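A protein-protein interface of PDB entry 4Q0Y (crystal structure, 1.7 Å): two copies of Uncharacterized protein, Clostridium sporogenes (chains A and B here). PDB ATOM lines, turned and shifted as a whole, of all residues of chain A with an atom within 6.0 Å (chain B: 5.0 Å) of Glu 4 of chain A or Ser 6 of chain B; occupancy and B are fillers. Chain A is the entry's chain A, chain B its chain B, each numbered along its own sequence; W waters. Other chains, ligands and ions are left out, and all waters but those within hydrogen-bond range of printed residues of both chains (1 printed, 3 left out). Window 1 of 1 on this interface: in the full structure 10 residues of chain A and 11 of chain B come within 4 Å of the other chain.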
ATOM      1  N   GLY A   1       7.679  16.152  17.798  1.00  0.00           N
ATOM      2  CA  GLY A   1       8.639  15.151  18.355  1.00  0.00           C
ATOM      3  C   GLY A   1      10.106  15.507  18.133  1.00  0.00           C
ATOM      4  O   GLY A   1      10.885  14.707  17.601  1.00  0.00           O
ATOM      5  N   ARG A   2      10.486  16.721  18.521  1.00  0.00           N
ATOM      6  CA  ARG A   2      11.905  17.081  18.582  1.00  0.00           C
ATOM      7  C   ARG A   2      12.645  16.343  19.717  1.00  0.00           C
ATOM      8  O   ARG A   2      13.857  16.235  19.669  1.00  0.00           O
ATOM      9  CB  ARG A   2      12.079  18.591  18.728  1.00  0.00           C
ATOM     10  CG  ARG A   2      11.687  19.333  17.469  1.00  0.00           C
ATOM     11  CD  ARG A   2      12.084  20.794  17.535  1.00  0.00           C
ATOM     12  NE  ARG A   2      12.140  21.355  16.187  1.00  0.00           N
ATOM     13  CZ  ARG A   2      11.086  21.685  15.434  1.00  0.00           C
ATOM     14  NH1 ARG A   2       9.821  21.540  15.863  1.00  0.00           N
ATOM     15  NH2 ARG A   2      11.302  22.173  14.219  1.00  0.00           N
ATOM     16  N   MET A   3      11.912  15.879  20.730  1.00  0.00           N
ATOM     17  CA  MET A   3      12.455  15.108  21.850  1.00  0.00           C
ATOM     18  C   MET A   3      11.724  13.808  21.950  1.00  0.00           C
ATOM     19  O   MET A   3      10.507  13.798  22.109  1.00  0.00           O
ATOM     20  CB  MET A   3      12.263  15.873  23.126  1.00  0.00           C
ATOM     21  CG  MET A   3      13.106  17.127  23.038  1.00  0.00           C
ATOM     22  SD  MET A   3      12.714  18.329  24.518  1.00  0.00           S
ATOM     23  CE  MET A   3      13.586  17.367  25.993  1.00  0.00           C
ATOM     24  N   GLU A   4      12.459  12.714  21.772  1.00  0.00           N
ATOM     25  CA  GLU A   4      11.891  11.375  21.697  1.00  0.00           C
ATOM     26  C   GLU A   4      12.597  10.476  22.678  1.00  0.00           C
ATOM     27  O   GLU A   4      13.802  10.339  22.592  1.00  0.00           O
ATOM     28  CB  GLU A   4      12.128  10.825  20.291  1.00  0.00           C
ATOM     29  CG  GLU A   4      11.394  11.568  19.203  1.00  0.00           C
ATOM     30  CD  GLU A   4       9.937  11.176  19.070  1.00  0.00           C
ATOM     31  OE1 GLU A   4       9.472  10.183  19.699  1.00  0.00           O
ATOM     32  OE2 GLU A   4       9.228  11.841  18.271  1.00  0.00           O
ATOM     33  N   ILE A   5      11.862   9.890  23.618  1.00  0.00           N
ATOM     34  CA  ILE A   5      12.464   8.975  24.610  1.00  0.00           C
ATOM     35  C   ILE A   5      12.854   7.713  23.867  1.00  0.00           C
ATOM     36  O   ILE A   5      12.031   7.131  23.163  1.00  0.00           O
ATOM     37  CB  ILE A   5      11.508   8.615  25.755  1.00  0.00           C
ATOM     38  CG1 ILE A   5      11.061   9.877  26.519  1.00  0.00           C
ATOM     39  CG2 ILE A   5      12.182   7.612  26.693  1.00  0.00           C
ATOM     40  CD1 ILE A   5       9.817   9.675  27.352  1.00  0.00           C
ATOM     41  N   SER A   6      14.118   7.317  23.988  1.00  0.00           N
ATOM     42  CA  SER A   6      14.628   6.097  23.331  1.00  0.00           C
ATOM     43  C   SER A   6      14.573   4.890  24.253  1.00  0.00           C
ATOM     44  O   SER A   6      14.371   3.790  23.763  1.00  0.00           O
ATOM     45  CB  SER A   6      16.043   6.286  22.779  1.00  0.00           C
ATOM     46  OG  SER A   6      16.881   6.843  23.728  1.00  0.00           O
ATOM     47  N   ASN A  44       5.874   8.959  25.039  1.00  0.00           N
ATOM     48  CA  ASN A  44       6.086   9.442  23.669  1.00  0.00           C
ATOM     49  C   ASN A  44       4.801   9.695  22.880  1.00  0.00           C
ATOM     50  O   ASN A  44       4.880  10.217  21.780  1.00  0.00           O
ATOM     51  CB  ASN A  44       6.976   8.443  22.860  1.00  0.00           C
ATOM     52  CG  ASN A  44       8.458   8.517  23.211  1.00  0.00           C
ATOM     53  OD1 ASN A  44       8.951   9.536  23.666  1.00  0.00           O
ATOM     54  ND2 ASN A  44       9.176   7.433  22.942  1.00  0.00           N
ATOM     55  N   LYS A  77      16.764   7.819  28.611  1.00  0.00           N
ATOM     56  CA  LYS A  77      17.586   8.397  27.534  1.00  0.00           C
ATOM     57  C   LYS A  77      16.652   8.914  26.468  1.00  0.00           C
ATOM     58  O   LYS A  77      15.632   8.285  26.207  1.00  0.00           O
ATOM     59  CB  LYS A  77      18.526   7.377  26.926  1.00  0.00           C
ATOM     60  CG  LYS A  77      19.541   6.887  27.919  1.00  0.00           C
ATOM     61  CD  LYS A  77      20.511   5.883  27.310  1.00  0.00           C
ATOM     62  CE  LYS A  77      21.412   5.251  28.355  1.00  0.00           C
ATOM     63  NZ  LYS A  77      22.344   4.253  27.771  1.00  0.00           N
ATOM     64  N   TYR A  78      16.950  10.088  25.893  1.00  0.00           N
ATOM     65  CA  TYR A  78      16.159  10.639  24.796  1.00  0.00           C
ATOM     66  C   TYR A  78      17.015  11.201  23.695  1.00  0.00           C
ATOM     67  O   TYR A  78      18.181  11.482  23.929  1.00  0.00           O
ATOM     68  CB  TYR A  78      15.151  11.681  25.300  1.00  0.00           C
ATOM     69  CG  TYR A  78      15.728  12.922  25.858  1.00  0.00           C
ATOM     70  CD1 TYR A  78      16.238  12.959  27.171  1.00  0.00           C
ATOM     71  CD2 TYR A  78      15.765  14.099  25.096  1.00  0.00           C
ATOM     72  CE1 TYR A  78      16.765  14.132  27.704  1.00  0.00           C
ATOM     73  CE2 TYR A  78      16.314  15.259  25.622  1.00  0.00           C
ATOM     74  CZ  TYR A  78      16.799  15.271  26.921  1.00  0.00           C
ATOM     75  OH  TYR A  78      17.351  16.413  27.437  1.00  0.00           O
ATOM     76  N   VAL A  79      16.432  11.319  22.494  1.00  0.00           N
ATOM     77  CA  VAL A  79      17.093  11.852  21.330  1.00  0.00           C
ATOM     78  C   VAL A  79      16.584  13.272  21.056  1.00  0.00           C
ATOM     79  O   VAL A  79      15.381  13.504  20.998  1.00  0.00           O
ATOM     80  CB  VAL A  79      16.889  10.994  20.061  1.00  0.00           C
ATOM     81  CG1 VAL A  79      17.523  11.656  18.844  1.00  0.00           C
ATOM     82  CG2 VAL A  79      17.469   9.609  20.272  1.00  0.00           C
ATOM     83  N   GLU A  80      17.517  14.185  20.885  1.00  0.00           N
ATOM     84  CA  GLU A  80      17.242  15.554  20.443  1.00  0.00           C
ATOM     85  C   GLU A  80      18.493  16.047  19.735  1.00  0.00           C
ATOM     86  O   GLU A  80      19.619  15.841  20.220  1.00  0.00           O
ATOM     87  CB  GLU A  80      16.891  16.443  21.639  1.00  0.00           C
ATOM     88  CG  GLU A  80      16.642  17.914  21.342  1.00  0.00           C
ATOM     89  CD  GLU A  80      16.425  18.768  22.590  1.00  0.00           C
ATOM     90  OE1 GLU A  80      15.995  18.264  23.633  1.00  0.00           O
ATOM     91  OE2 GLU A  80      16.686  19.983  22.520  1.00  0.00           O
ATOM     92  N   GLU B   4      16.902   0.790  17.928  1.00  0.00           N
ATOM     93  CA  GLU B   4      15.523   1.252  18.217  1.00  0.00           C
ATOM     94  C   GLU B   4      15.225   2.512  17.396  1.00  0.00           C
ATOM     95  O   GLU B   4      16.049   3.440  17.467  1.00  0.00           O
ATOM     96  CB  GLU B   4      15.392   1.604  19.731  1.00  0.00           C
ATOM     97  CG  GLU B   4      13.947   1.672  20.268  1.00  0.00           C
ATOM     98  CD  GLU B   4      13.289   0.303  20.447  1.00  0.00           C
ATOM     99  OE1 GLU B   4      13.903  -0.753  20.171  1.00  0.00           O
ATOM    100  OE2 GLU B   4      12.136   0.271  20.899  1.00  0.00           O
ATOM    101  N   ILE B   5      14.053   2.575  16.718  1.00  0.00           N
ATOM    102  CA  ILE B   5      13.629   3.771  15.972  1.00  0.00           C
ATOM    103  C   ILE B   5      13.258   4.835  16.980  1.00  0.00           C
ATOM    104  O   ILE B   5      12.377   4.619  17.834  1.00  0.00           O
ATOM    105  CB  ILE B   5      12.409   3.570  15.043  1.00  0.00           C
ATOM    106  CG1 ILE B   5      12.686   2.475  14.008  1.00  0.00           C
ATOM    107  CG2 ILE B   5      12.038   4.888  14.316  1.00  0.00           C
ATOM    108  CD1 ILE B   5      11.441   1.948  13.315  1.00  0.00           C
ATOM    109  N   SER B   6      13.919   5.982  16.882  1.00  0.00           N
ATOM    110  CA  SER B   6      13.637   7.111  17.771  1.00  0.00           C
ATOM    111  C   SER B   6      12.629   8.056  17.167  1.00  0.00           C
ATOM    112  O   SER B   6      11.853   8.668  17.917  1.00  0.00           O
ATOM    113  CB  SER B   6      14.894   7.892  18.174  1.00  0.00           C
ATOM    114  OG  SER B   6      15.660   8.218  17.040  1.00  0.00           O
ATOM    115  N   SER B   7      12.675   8.243  15.844  1.00  0.00           N
ATOM    116  CA  SER B   7      11.738   9.150  15.161  1.00  0.00           C
ATOM    117  C   SER B   7      11.645   8.832  13.683  1.00  0.00           C
ATOM    118  O   SER B   7      12.584   8.245  13.120  1.00  0.00           O
ATOM    119  CB  SER B   7      12.160  10.613  15.347  1.00  0.00           C
ATOM    120  OG  SER B   7      13.446  10.897  14.775  1.00  0.00           O
ATOM    121  N   LEU B   8      10.519   9.212  13.069  1.00  0.00           N
ATOM    122  CA  LEU B   8      10.351   9.220  11.606  1.00  0.00           C
ATOM    123  C   LEU B   8      10.191  10.648  11.157  1.00  0.00           C
ATOM    124  O   LEU B   8       9.459  11.402  11.790  1.00  0.00           O
ATOM    125  CB  LEU B   8       9.086   8.493  11.169  1.00  0.00           C
ATOM    126  CG  LEU B   8       9.194   6.994  10.988  1.00  0.00           C
ATOM    127  CD1 LEU B   8       9.613   6.290  12.249  1.00  0.00           C
ATOM    128  CD2 LEU B   8       7.847   6.492  10.511  1.00  0.00           C
ATOM    129  N   GLU B  33       2.944  14.726  11.885  1.00  0.00           N
ATOM    130  CA  GLU B  33       3.583  14.235  13.122  1.00  0.00           C
ATOM    131  C   GLU B  33       2.833  13.083  13.817  1.00  0.00           C
ATOM    132  O   GLU B  33       3.452  12.064  14.198  1.00  0.00           O
ATOM    133  CB  GLU B  33       3.787  15.397  14.097  1.00  0.00           C
ATOM    134  CG  GLU B  33       4.629  15.097  15.321  1.00  0.00           C
ATOM    135  CD  GLU B  33       6.062  14.711  15.007  1.00  0.00           C
ATOM    136  OE1 GLU B  33       6.549  14.938  13.862  1.00  0.00           O
ATOM    137  OE2 GLU B  33       6.755  14.191  15.927  1.00  0.00           O
ATOM    138  N   LYS B  40       5.629   4.742  13.823  1.00  0.00           N
ATOM    139  CA  LYS B  40       6.825   4.416  14.634  1.00  0.00           C
ATOM    140  C   LYS B  40       6.504   3.340  15.664  1.00  0.00           C
ATOM    141  O   LYS B  40       7.264   2.385  15.830  1.00  0.00           O
ATOM    142  CB  LYS B  40       7.381   5.654  15.348  1.00  0.00           C
ATOM    143  CG  LYS B  40       8.666   5.382  16.134  1.00  0.00           C
ATOM    144  CD  LYS B  40       9.110   6.601  16.945  1.00  0.00           C
ATOM    145  CE  LYS B  40       8.949   6.415  18.433  1.00  0.00           C
ATOM    146  NZ  LYS B  40       9.540   7.543  19.204  1.00  0.00           N
ATOM    147  N   LYS B  77      15.223   7.988  12.112  1.00  0.00           N
ATOM    148  CA  LYS B  77      16.439   8.009  12.947  1.00  0.00           C
ATOM    149  C   LYS B  77      16.330   6.862  13.908  1.00  0.00           C
ATOM    150  O   LYS B  77      15.222   6.589  14.399  1.00  0.00           O
ATOM    151  CB  LYS B  77      16.590   9.308  13.728  1.00  0.00           C
ATOM    152  CG  LYS B  77      16.760  10.472  12.800  1.00  0.00           C
ATOM    153  CD  LYS B  77      16.923  11.812  13.477  1.00  0.00           C
ATOM    154  CE  LYS B  77      17.090  12.850  12.358  1.00  0.00           C
ATOM    155  NZ  LYS B  77      18.510  12.995  11.914  1.00  0.00           N
ATOM    156  N   TYR B  78      17.469   6.221  14.193  1.00  0.00           N
ATOM    157  CA  TYR B  78      17.550   5.181  15.200  1.00  0.00           C
ATOM    158  C   TYR B  78      18.764   5.302  16.086  1.00  0.00           C
ATOM    159  O   TYR B  78      19.751   5.944  15.725  1.00  0.00           O
ATOM    160  CB  TYR B  78      17.459   3.815  14.515  1.00  0.00           C
ATOM    161  CG  TYR B  78      18.623   3.457  13.622  1.00  0.00           C
ATOM    162  CD1 TYR B  78      18.665   3.887  12.280  1.00  0.00           C
ATOM    163  CD2 TYR B  78      19.667   2.673  14.099  1.00  0.00           C
ATOM    164  CE1 TYR B  78      19.727   3.537  11.448  1.00  0.00           C
ATOM    165  CE2 TYR B  78      20.753   2.320  13.279  1.00  0.00           C
ATOM    166  CZ  TYR B  78      20.771   2.759  11.946  1.00  0.00           C
ATOM    167  OH  TYR B  78      21.833   2.437  11.116  1.00  0.00           O
ATOM    168  N   VAL B  79      18.679   4.679  17.265  1.00  0.00           N
ATOM    169  CA  VAL B  79      19.724   4.724  18.258  1.00  0.00           C
ATOM    170  C   VAL B  79      20.409   3.359  18.286  1.00  0.00           C
ATOM    171  O   VAL B  79      19.730   2.330  18.322  1.00  0.00           O
ATOM    172  CB  VAL B  79      19.182   5.074  19.659  1.00  0.00           C
ATOM    173  CG1 VAL B  79      20.238   4.902  20.728  1.00  0.00           C
ATOM    174  CG2 VAL B  79      18.648   6.501  19.669  1.00  0.00           C
ATOM    175  N   VAL B  84      23.059   8.381  17.387  1.00  0.00           N
ATOM    176  CA  VAL B  84      21.898   8.515  16.523  1.00  0.00           C
ATOM    177  C   VAL B  84      22.349   8.334  15.062  1.00  0.00           C
ATOM    178  O   VAL B  84      23.379   8.904  14.663  1.00  0.00           O
ATOM    179  CB  VAL B  84      21.172   9.871  16.756  1.00  0.00           C
ATOM    180  CG1 VAL B  84      19.908   9.972  15.891  1.00  0.00           C
ATOM    181  CG2 VAL B  84      20.824  10.049  18.244  1.00  0.00           C
HETATM  182  O   HOH W   1      11.500   5.883  20.706  1.00  0.00           O
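The side-chain carboxylate of Glu 33 of chain B lies close to the backbone NH of Gly 1 of chain A, at 2.9 Å.
The side-chain carboxylate (OE1) of Glu 4 of chain A lies close to the side-chain amino group (NZ) of Lys 40 of chain B, 2.7 Å away.
OE1 of Glu 4 of chain A lies close to O of Ser 6 of chain B, 3.3 Å away.
The backbone carbonyl oxygen (O) of Glu 4 of chain A lies within hydrogen-bond range of the backbone NH (N) of Val 79 of chain A (2.8 Å).
ND2 of Asn 44 of chain A lies within hydrogen-bond range of O of Ile 5 of chain A.
O of Glu 4 of chain B is in hydrogen-bond range of N of Val 79 of chain B, at 2.9 Å.
O of Ser 6 of chain B lies within hydrogen-bond range of NZ of Lys 40 of chain B.
The backbone NH (N) of Ser 6 of chain B lies within hydrogen-bond range of the backbone carbonyl oxygen (O) of Lys 77 of chain B (2.9 Å).
Among the printed residues, merely in contact across the chains: Val 79 of chain A with Val 79 of chain B, Val 79 of chain A with Val 84 of chain B, Val 79 of chain A with Ser 6 of chain B and Asn 44 of chain A with Lys 40 of chain B.
Of chain A, only Glu 4 (3.2 Å) and Val 79 (3.7 Å) come within 4 Å of Ser 6 of chain B.
Of the printed residues of chain A, Lys 40 of chain B touches Glu 4 and Asn 44.
Of the printed residues of chain B, Gly 1 of chain A touches Glu 33 (2.9 Å).
Arg 2 of chain A touches none of the printed residues of chain B.
Ser 7 of chain B touches none of the printed residues of chain A.
The nearest residue of chain B that does not touch Glu 4 of chain A is Ser 7 of chain B (4.05 Å).
The nearest residue of chain A that does not touch Ser 6 of chain B is Ser 6 of chain A (5.0 Å).
The nearest printed residue of chain B that does not touch Asn 44 of chain A is Ser 6 of chain B (5.8 Å).
Of the 11 printed residues of chain B, 5 touch a printed residue of chain A.
Printed residues of chain B that touch a printed residue of chain A: Ser 6, Glu 33, Lys 40, Val 79 and Val 84.
Hydrophobic or aromatic side chains of chain B that line the printed part of chain A: Val 79 and Val 84.
Printed residues of chain A that touch a printed residue of chain B: Gly 1, Glu 4, Asn 44 and Val 79.
Hydrophobic or aromatic side chains of chain A within 4 Å of the printed part of chain B: Val 79.
Glu 4 of chain A touches Ser 6 of chain B, but with the chains exchanged Ser 6 of chain A does not touch Glu 4 of chain B (4.1 Å).
Val 79 of chain A touches Ser 6 of chain B, but with the chains exchanged Ser 6 of chain A does not touch Val 79 of chain B (4.1 Å).
Val 79 of chain A touches its own counterpart, Val 79 of chain B.
Water W1 lies within hydrogen-bond range of O of Ile 5 of chain A, NZ of Lys 40 of chain B and O of Ile 5 of chain B.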
